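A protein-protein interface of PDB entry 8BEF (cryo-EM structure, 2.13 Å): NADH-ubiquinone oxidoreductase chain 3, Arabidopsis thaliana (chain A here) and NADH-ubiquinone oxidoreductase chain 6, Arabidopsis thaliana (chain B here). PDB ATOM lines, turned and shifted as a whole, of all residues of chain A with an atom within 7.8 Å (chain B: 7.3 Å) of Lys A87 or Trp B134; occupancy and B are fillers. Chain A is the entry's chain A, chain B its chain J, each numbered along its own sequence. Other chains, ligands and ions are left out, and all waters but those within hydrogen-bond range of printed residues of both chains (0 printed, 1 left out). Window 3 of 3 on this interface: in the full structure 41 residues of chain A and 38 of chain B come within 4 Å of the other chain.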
ATOM      1  N   FME A   1      -9.785  -2.430  14.911  1.00  0.00           N
ATOM      2  CN  FME A   1      -9.552  -3.570  15.646  1.00  0.00           C
ATOM      3  O1  FME A   1      -9.173  -3.565  16.825  1.00  0.00           O
ATOM      4  CA  FME A   1      -9.626  -1.105  15.442  1.00  0.00           C
ATOM      5  CB  FME A   1      -9.800  -0.001  14.376  1.00  0.00           C
ATOM      6  CG  FME A   1      -9.095  -0.340  13.091  1.00  0.00           C
ATOM      7  SD  FME A   1      -7.351  -0.270  13.402  1.00  0.00           S
ATOM      8  CE  FME A   1      -7.104   1.410  13.832  1.00  0.00           C
ATOM      9  C   FME A   1     -10.618  -0.802  16.562  1.00  0.00           C
ATOM     10  O   FME A   1     -11.927  -0.933  16.224  1.00  0.00           O
ATOM     11  N   PRO A  80     -18.895 -16.571  19.300  1.00  0.00           N
ATOM     12  CA  PRO A  80     -17.792 -16.921  18.385  1.00  0.00           C
ATOM     13  C   PRO A  80     -18.148 -18.048  17.437  1.00  0.00           C
ATOM     14  O   PRO A  80     -17.739 -18.030  16.273  1.00  0.00           O
ATOM     15  CB  PRO A  80     -16.651 -17.322  19.336  1.00  0.00           C
ATOM     16  CG  PRO A  80     -17.057 -16.841  20.680  1.00  0.00           C
ATOM     17  CD  PRO A  80     -18.548 -16.906  20.691  1.00  0.00           C
ATOM     18  N   TRP A  81     -18.916 -19.027  17.917  1.00  0.00           N
ATOM     19  CA  TRP A  81     -19.349 -20.134  17.072  1.00  0.00           C
ATOM     20  C   TRP A  81     -20.165 -19.626  15.892  1.00  0.00           C
ATOM     21  O   TRP A  81     -19.941 -20.023  14.740  1.00  0.00           O
ATOM     22  CB  TRP A  81     -20.157 -21.119  17.920  1.00  0.00           C
ATOM     23  CG  TRP A  81     -20.689 -22.315  17.202  1.00  0.00           C
ATOM     24  CD1 TRP A  81     -19.989 -23.425  16.832  1.00  0.00           C
ATOM     25  CD2 TRP A  81     -22.043 -22.545  16.805  1.00  0.00           C
ATOM     26  NE1 TRP A  81     -20.817 -24.323  16.213  1.00  0.00           N
ATOM     27  CE2 TRP A  81     -22.087 -23.810  16.187  1.00  0.00           C
ATOM     28  CE3 TRP A  81     -23.223 -21.803  16.905  1.00  0.00           C
ATOM     29  CZ2 TRP A  81     -23.263 -24.347  15.672  1.00  0.00           C
ATOM     30  CZ3 TRP A  81     -24.387 -22.339  16.396  1.00  0.00           C
ATOM     31  CH2 TRP A  81     -24.399 -23.598  15.783  1.00  0.00           C
ATOM     32  N   VAL A  83     -20.158 -16.642  14.511  1.00  0.00           N
ATOM     33  CA  VAL A  83     -19.371 -15.962  13.483  1.00  0.00           C
ATOM     34  C   VAL A  83     -18.347 -16.882  12.819  1.00  0.00           C
ATOM     35  O   VAL A  83     -17.816 -16.533  11.759  1.00  0.00           O
ATOM     36  CB  VAL A  83     -18.672 -14.705  14.028  1.00  0.00           C
ATOM     37  CG1 VAL A  83     -19.697 -13.752  14.630  1.00  0.00           C
ATOM     38  CG2 VAL A  83     -17.596 -15.074  15.035  1.00  0.00           C
ATOM     39  N   SER A  84     -18.056 -18.043  13.400  1.00  0.00           N
ATOM     40  CA  SER A  84     -17.014 -18.924  12.886  1.00  0.00           C
ATOM     41  C   SER A  84     -17.544 -20.135  12.127  1.00  0.00           C
ATOM     42  O   SER A  84     -16.742 -20.965  11.692  1.00  0.00           O
ATOM     43  CB  SER A  84     -16.122 -19.401  14.036  1.00  0.00           C
ATOM     44  OG  SER A  84     -15.477 -18.309  14.661  1.00  0.00           O
ATOM     45  N   LEU A  85     -18.864 -20.261  11.967  1.00  0.00           N
ATOM     46  CA  LEU A  85     -19.420 -21.451  11.322  1.00  0.00           C
ATOM     47  C   LEU A  85     -18.841 -21.695   9.931  1.00  0.00           C
ATOM     48  O   LEU A  85     -18.690 -22.853   9.524  1.00  0.00           O
ATOM     49  CB  LEU A  85     -20.941 -21.339  11.242  1.00  0.00           C
ATOM     50  CG  LEU A  85     -21.714 -21.973  12.401  1.00  0.00           C
ATOM     51  CD1 LEU A  85     -23.208 -21.919  12.136  1.00  0.00           C
ATOM     52  CD2 LEU A  85     -21.260 -23.409  12.643  1.00  0.00           C
ATOM     53  N   ASN A  86     -18.509 -20.635   9.189  1.00  0.00           N
ATOM     54  CA  ASN A  86     -18.013 -20.824   7.829  1.00  0.00           C
ATOM     55  C   ASN A  86     -16.646 -21.500   7.808  1.00  0.00           C
ATOM     56  O   ASN A  86     -16.288 -22.132   6.809  1.00  0.00           O
ATOM     57  CB  ASN A  86     -17.952 -19.487   7.083  1.00  0.00           C
ATOM     58  CG  ASN A  86     -17.246 -18.394   7.872  1.00  0.00           C
ATOM     59  OD1 ASN A  86     -16.689 -18.632   8.942  1.00  0.00           O
ATOM     60  ND2 ASN A  86     -17.277 -17.180   7.339  1.00  0.00           N
ATOM     61  N   LYS A  87     -15.876 -21.391   8.886  1.00  0.00           N
ATOM     62  CA  LYS A  87     -14.539 -21.969   8.922  1.00  0.00           C
ATOM     63  C   LYS A  87     -14.456 -23.287   9.683  1.00  0.00           C
ATOM     64  O   LYS A  87     -13.645 -24.142   9.318  1.00  0.00           O
ATOM     65  CB  LYS A  87     -13.554 -20.969   9.530  1.00  0.00           C
ATOM     66  CG  LYS A  87     -13.232 -19.813   8.601  1.00  0.00           C
ATOM     67  CD  LYS A  87     -12.101 -18.961   9.139  1.00  0.00           C
ATOM     68  CE  LYS A  87     -12.405 -18.499  10.546  1.00  0.00           C
ATOM     69  NZ  LYS A  87     -13.209 -17.247  10.553  1.00  0.00           N
ATOM     70  N   ILE A  88     -15.267 -23.481  10.725  1.00  0.00           N
ATOM     71  CA  ILE A  88     -15.156 -24.702  11.516  1.00  0.00           C
ATOM     72  C   ILE A  88     -15.912 -25.870  10.899  1.00  0.00           C
ATOM     73  O   ILE A  88     -15.604 -27.025  11.213  1.00  0.00           O
ATOM     74  CB  ILE A  88     -15.641 -24.476  12.958  1.00  0.00           C
ATOM     75  CG1 ILE A  88     -17.126 -24.098  12.978  1.00  0.00           C
ATOM     76  CG2 ILE A  88     -14.783 -23.434  13.645  1.00  0.00           C
ATOM     77  CD1 ILE A  88     -17.603 -23.561  14.307  1.00  0.00           C
ATOM     78  N   ASP A  89     -16.903 -25.599  10.058  1.00  0.00           N
ATOM     79  CA  ASP A  89     -17.600 -26.595   9.222  1.00  0.00           C
ATOM     80  C   ASP A  89     -18.271 -27.637  10.126  1.00  0.00           C
ATOM     81  O   ASP A  89     -18.856 -27.279  11.160  1.00  0.00           O
ATOM     82  CB  ASP A  89     -16.637 -27.165   8.209  1.00  0.00           C
ATOM     83  CG  ASP A  89     -17.347 -27.787   7.025  1.00  0.00           C
ATOM     84  OD1 ASP A  89     -18.589 -27.676   6.956  1.00  0.00           O
ATOM     85  OD2 ASP A  89     -16.665 -28.385   6.166  1.00  0.00           O
ATOM     86  N   LEU A  90     -18.209 -28.921   9.765  1.00  0.00           N
ATOM     87  CA  LEU A  90     -19.023 -29.931  10.434  1.00  0.00           C
ATOM     88  C   LEU A  90     -18.509 -30.237  11.835  1.00  0.00           C
ATOM     89  O   LEU A  90     -19.303 -30.456  12.755  1.00  0.00           O
ATOM     90  CB  LEU A  90     -19.070 -31.204   9.591  1.00  0.00           C
ATOM     91  CG  LEU A  90     -20.094 -31.192   8.458  1.00  0.00           C
ATOM     92  CD1 LEU A  90     -20.046 -32.490   7.671  1.00  0.00           C
ATOM     93  CD2 LEU A  90     -21.490 -30.936   9.005  1.00  0.00           C
ATOM     94  N   PHE A  91     -17.188 -30.270  12.012  1.00  0.00           N
ATOM     95  CA  PHE A  91     -16.620 -30.599  13.316  1.00  0.00           C
ATOM     96  C   PHE A  91     -17.051 -29.590  14.373  1.00  0.00           C
ATOM     97  O   PHE A  91     -17.461 -29.970  15.476  1.00  0.00           O
ATOM     98  CB  PHE A  91     -15.093 -30.664  13.220  1.00  0.00           C
ATOM     99  CG  PHE A  91     -14.440 -31.365  14.374  1.00  0.00           C
ATOM    100  CD1 PHE A  91     -14.324 -30.744  15.608  1.00  0.00           C
ATOM    101  CD2 PHE A  91     -13.931 -32.645  14.224  1.00  0.00           C
ATOM    102  CE1 PHE A  91     -13.722 -31.384  16.668  1.00  0.00           C
ATOM    103  CE2 PHE A  91     -13.323 -33.289  15.281  1.00  0.00           C
ATOM    104  CZ  PHE A  91     -13.223 -32.661  16.504  1.00  0.00           C
ATOM    105  N   GLY A  92     -16.958 -28.297  14.056  1.00  0.00           N
ATOM    106  CA  GLY A  92     -17.368 -27.280  15.011  1.00  0.00           C
ATOM    107  C   GLY A  92     -18.853 -27.336  15.310  1.00  0.00           C
ATOM    108  O   GLY A  92     -19.276 -27.160  16.459  1.00  0.00           O
ATOM    109  N   GLY B 129      -0.646  -8.534   6.394  1.00  0.00           N
ATOM    110  CA  GLY B 129      -1.581  -8.952   7.421  1.00  0.00           C
ATOM    111  C   GLY B 129      -2.822  -8.092   7.535  1.00  0.00           C
ATOM    112  O   GLY B 129      -3.717  -8.434   8.315  1.00  0.00           O
ATOM    113  N   ARG B 132      -7.014  -8.854   5.111  1.00  0.00           N
ATOM    114  CA  ARG B 132      -8.186  -9.486   5.728  1.00  0.00           C
ATOM    115  C   ARG B 132      -7.920  -9.614   7.221  1.00  0.00           C
ATOM    116  O   ARG B 132      -7.410 -10.640   7.677  1.00  0.00           O
ATOM    117  CB  ARG B 132      -8.477 -10.843   5.106  1.00  0.00           C
ATOM    118  CG  ARG B 132      -9.696 -11.549   5.682  1.00  0.00           C
ATOM    119  CD  ARG B 132      -9.980 -12.843   4.988  1.00  0.00           C
ATOM    120  NE  ARG B 132     -11.155 -13.537   5.498  1.00  0.00           N
ATOM    121  CZ  ARG B 132     -11.705 -14.592   4.919  1.00  0.00           C
ATOM    122  NH1 ARG B 132     -11.212 -15.096   3.797  1.00  0.00           N
ATOM    123  NH2 ARG B 132     -12.763 -15.166   5.483  1.00  0.00           N
ATOM    124  N   SER B 133      -8.298  -8.588   7.976  1.00  0.00           N
ATOM    125  CA  SER B 133      -8.085  -8.604   9.414  1.00  0.00           C
ATOM    126  C   SER B 133      -9.179  -9.410  10.103  1.00  0.00           C
ATOM    127  O   SER B 133     -10.336  -9.403   9.680  1.00  0.00           O
ATOM    128  CB  SER B 133      -8.048  -7.179   9.969  1.00  0.00           C
ATOM    129  OG  SER B 133      -9.095  -6.395   9.420  1.00  0.00           O
ATOM    130  N   TRP B 134      -8.795 -10.120  11.156  1.00  0.00           N
ATOM    131  CA  TRP B 134      -9.715 -10.925  11.945  1.00  0.00           C
ATOM    132  C   TRP B 134     -10.107 -10.176  13.210  1.00  0.00           C
ATOM    133  O   TRP B 134      -9.259  -9.577  13.875  1.00  0.00           O
ATOM    134  CB  TRP B 134      -9.085 -12.267  12.327  1.00  0.00           C
ATOM    135  CG  TRP B 134      -9.171 -13.320  11.271  1.00  0.00           C
ATOM    136  CD1 TRP B 134      -9.387 -13.132   9.935  1.00  0.00           C
ATOM    137  CD2 TRP B 134      -9.040 -14.736  11.460  1.00  0.00           C
ATOM    138  NE1 TRP B 134      -9.402 -14.343   9.283  1.00  0.00           N
ATOM    139  CE2 TRP B 134      -9.191 -15.342  10.198  1.00  0.00           C
ATOM    140  CE3 TRP B 134      -8.816 -15.547  12.577  1.00  0.00           C
ATOM    141  CZ2 TRP B 134      -9.118 -16.724  10.020  1.00  0.00           C
ATOM    142  CZ3 TRP B 134      -8.745 -16.917  12.398  1.00  0.00           C
ATOM    143  CH2 TRP B 134      -8.893 -17.491  11.130  1.00  0.00           C
ATOM    144  N   THR B 135     -11.392 -10.221  13.544  1.00  0.00           N
ATOM    145  CA  THR B 135     -11.819  -9.728  14.843  1.00  0.00           C
ATOM    146  C   THR B 135     -11.344 -10.670  15.951  1.00  0.00           C
ATOM    147  O   THR B 135     -11.022 -11.838  15.716  1.00  0.00           O
ATOM    148  CB  THR B 135     -13.343  -9.577  14.896  1.00  0.00           C
ATOM    149  OG1 THR B 135     -13.958 -10.870  14.944  1.00  0.00           O
ATOM    150  CG2 THR B 135     -13.851  -8.818  13.675  1.00  0.00           C
ATOM    151  N   ASN B 136     -11.283 -10.131  17.170  1.00  0.00           N
ATOM    152  CA  ASN B 136     -11.038 -10.956  18.351  1.00  0.00           C
ATOM    153  C   ASN B 136     -12.020 -12.123  18.403  1.00  0.00           C
ATOM    154  O   ASN B 136     -11.636 -13.268  18.684  1.00  0.00           O
ATOM    155  CB  ASN B 136     -11.146 -10.074  19.602  1.00  0.00           C
ATOM    156  CG  ASN B 136     -10.887 -10.828  20.896  1.00  0.00           C
ATOM    157  OD1 ASN B 136     -11.390 -10.445  21.949  1.00  0.00           O
ATOM    158  ND2 ASN B 136     -10.093 -11.889  20.828  1.00  0.00           N
ATOM    159  N   LEU B 137     -13.283 -11.847  18.071  1.00  0.00           N
ATOM    160  CA  LEU B 137     -14.333 -12.858  18.117  1.00  0.00           C
ATOM    161  C   LEU B 137     -14.033 -14.024  17.182  1.00  0.00           C
ATOM    162  O   LEU B 137     -14.082 -15.190  17.591  1.00  0.00           O
ATOM    163  CB  LEU B 137     -15.670 -12.206  17.761  1.00  0.00           C
ATOM    164  CG  LEU B 137     -16.966 -12.995  17.909  1.00  0.00           C
ATOM    165  CD1 LEU B 137     -17.099 -13.541  19.310  1.00  0.00           C
ATOM    166  CD2 LEU B 137     -18.160 -12.121  17.556  1.00  0.00           C
ATOM    167  N   GLU B 138     -13.711 -13.733  15.922  1.00  0.00           N
ATOM    168  CA  GLU B 138     -13.501 -14.822  14.976  1.00  0.00           C
ATOM    169  C   GLU B 138     -12.167 -15.530  15.190  1.00  0.00           C
ATOM    170  O   GLU B 138     -12.075 -16.737  14.943  1.00  0.00           O
ATOM    171  CB  GLU B 138     -13.660 -14.318  13.540  1.00  0.00           C
ATOM    172  CG  GLU B 138     -12.715 -13.243  13.082  1.00  0.00           C
ATOM    173  CD  GLU B 138     -13.395 -12.277  12.116  1.00  0.00           C
ATOM    174  OE1 GLU B 138     -14.584 -12.485  11.805  1.00  0.00           O
ATOM    175  OE2 GLU B 138     -12.750 -11.313  11.670  1.00  0.00           O
ATOM    176  N   THR B 139     -11.148 -14.830  15.698  1.00  0.00           N
ATOM    177  CA  THR B 139      -9.913 -15.516  16.070  1.00  0.00           C
ATOM    178  C   THR B 139     -10.154 -16.520  17.191  1.00  0.00           C
ATOM    179  O   THR B 139      -9.627 -17.637  17.155  1.00  0.00           O
ATOM    180  CB  THR B 139      -8.833 -14.506  16.470  1.00  0.00           C
ATOM    181  OG1 THR B 139      -8.762 -13.457  15.496  1.00  0.00           O
ATOM    182  CG2 THR B 139      -7.471 -15.190  16.573  1.00  0.00           C
ATOM    183  N   LEU B 140     -10.948 -16.144  18.199  1.00  0.00           N
ATOM    184  CA  LEU B 140     -11.268 -17.088  19.271  1.00  0.00           C
ATOM    185  C   LEU B 140     -12.133 -18.244  18.765  1.00  0.00           C
ATOM    186  O   LEU B 140     -11.907 -19.413  19.125  1.00  0.00           O
ATOM    187  CB  LEU B 140     -11.966 -16.349  20.412  1.00  0.00           C
ATOM    188  CG  LEU B 140     -12.090 -17.065  21.754  1.00  0.00           C
ATOM    189  CD1 LEU B 140     -10.758 -17.666  22.168  1.00  0.00           C
ATOM    190  CD2 LEU B 140     -12.604 -16.094  22.810  1.00  0.00           C
ATOM    191  N   GLY B 141     -13.127 -17.935  17.927  1.00  0.00           N
ATOM    192  CA  GLY B 141     -14.038 -18.952  17.435  1.00  0.00           C
ATOM    193  C   GLY B 141     -13.414 -19.912  16.450  1.00  0.00           C
ATOM    194  O   GLY B 141     -13.941 -21.011  16.253  1.00  0.00           O
ATOM    195  N   ASN B 142     -12.310 -19.516  15.816  1.00  0.00           N
ATOM    196  CA  ASN B 142     -11.542 -20.434  14.989  1.00  0.00           C
ATOM    197  C   ASN B 142     -10.930 -21.576  15.798  1.00  0.00           C
ATOM    198  O   ASN B 142     -10.585 -22.612  15.223  1.00  0.00           O
ATOM    199  CB  ASN B 142     -10.443 -19.652  14.266  1.00  0.00           C
ATOM    200  CG  ASN B 142      -9.653 -20.503  13.298  1.00  0.00           C
ATOM    201  OD1 ASN B 142     -10.220 -21.190  12.451  1.00  0.00           O
ATOM    202  ND2 ASN B 142      -8.334 -20.463  13.419  1.00  0.00           N
ATOM    203  N   LEU B 143     -10.786 -21.409  17.111  1.00  0.00           N
ATOM    204  CA  LEU B 143     -10.070 -22.363  17.947  1.00  0.00           C
ATOM    205  C   LEU B 143     -10.937 -23.103  18.948  1.00  0.00           C
ATOM    206  O   LEU B 143     -10.654 -24.267  19.237  1.00  0.00           O
ATOM    207  CB  LEU B 143      -8.956 -21.659  18.726  1.00  0.00           C
ATOM    208  CG  LEU B 143      -7.898 -20.945  17.895  1.00  0.00           C
ATOM    209  CD1 LEU B 143      -6.933 -20.237  18.821  1.00  0.00           C
ATOM    210  CD2 LEU B 143      -7.181 -21.941  17.006  1.00  0.00           C
ATOM    211  N   THR B 146     -12.859 -26.556  17.486  1.00  0.00           N
ATOM    212  CA  THR B 146     -12.195 -27.586  16.698  1.00  0.00           C
ATOM    213  C   THR B 146     -10.901 -28.081  17.331  1.00  0.00           C
ATOM    214  O   THR B 146     -10.830 -29.242  17.737  1.00  0.00           O
ATOM    215  CB  THR B 146     -11.942 -27.046  15.285  1.00  0.00           C
ATOM    216  OG1 THR B 146     -11.297 -25.772  15.374  1.00  0.00           O
ATOM    217  CG2 THR B 146     -13.255 -26.886  14.542  1.00  0.00           C
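The side-chain hydroxyl of Ser A84 sits close to the backbone carbonyl oxygen of Gly B141 (3.5 Å).
OG of Ser A84 is in hydrogen-bond range of O of Pro A80, 2.8 Å away.
The backbone carbonyl oxygen (O) of Gly A92 lies within hydrogen-bond range of the indole nitrogen (NE1) of Trp A81, 3.2 Å away.
The backbone NH (N) of Leu B137 sits close to the side-chain hydroxyl (OG1) of Thr B135 (3.3 Å).
N of Thr B135 is in hydrogen-bond range of OE2 of Glu B138, 2.6 Å away.
OG1 of Thr B146 sits at hydrogen-bond distance from O of Asn B142, at 3.2 Å.
N of Pro A80 touches CD1 of Leu B137, at 3.5 Å.
Pro A80 touches Gly B141 (CB to CA, 3.6 Å).
Leu B137 touches Val A83.
O of Glu B138 touches OG of Ser A84, at 3.8 Å.
Asn B142 touches Ser A84 (N to OG, 3.6 Å).
CE of Lys A87 touches CH2 of Trp B134, at 3.7 Å.
CE of Lys A87 touches OD1 of Asn B142, at 3.96 Å.
Ile A88 touches Gly B141.
Ile A88 touches Thr B146.
O of Thr B146 touches CE1 of Phe A91, 3.8 Å away.
Of chain B, only Trp B134 (3.7 Å) and Asn B142 (3.96 Å) come within 4 Å of Lys A87.
Printed residues of chain A within 4 Å of Asn B142: Ser A84 (3.6 Å) and Lys A87 (3.96 Å).
Printed residues of chain B within 4 Å of Gly A92: Thr B146.
Asn B136 touches none of the printed residues of chain A.
The nearest residue of chain B that does not touch Lys A87 is Glu B138 (4.2 Å).
The nearest printed residue of chain B that does not touch Pro A80 is Leu B140 (4.6 Å).
Hydrophobic or aromatic side chains of chain B within 4 Å of the printed part of chain A: Trp B134 and Leu B137.
Along chain B the printed residues that touch a printed residue of chain A span positions 134 to 146.
Printed residues of chain A that touch a printed residue of chain B: Pro A80, Val A83, Ser A84, Lys A87, Ile A88, Phe A91 and Gly A92.
Hydrophobic or aromatic side chains of chain A within 4 Å of the printed part of chain B: Pro A80, Val A83, Ile A88 and Phe A91.
Among the printed residues, 12 pairs touch across the chains.
Among the printed residues, no Asp or Glu carboxylate lies within 4 Å of a Lys or Arg side-chain nitrogen of the other chain.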
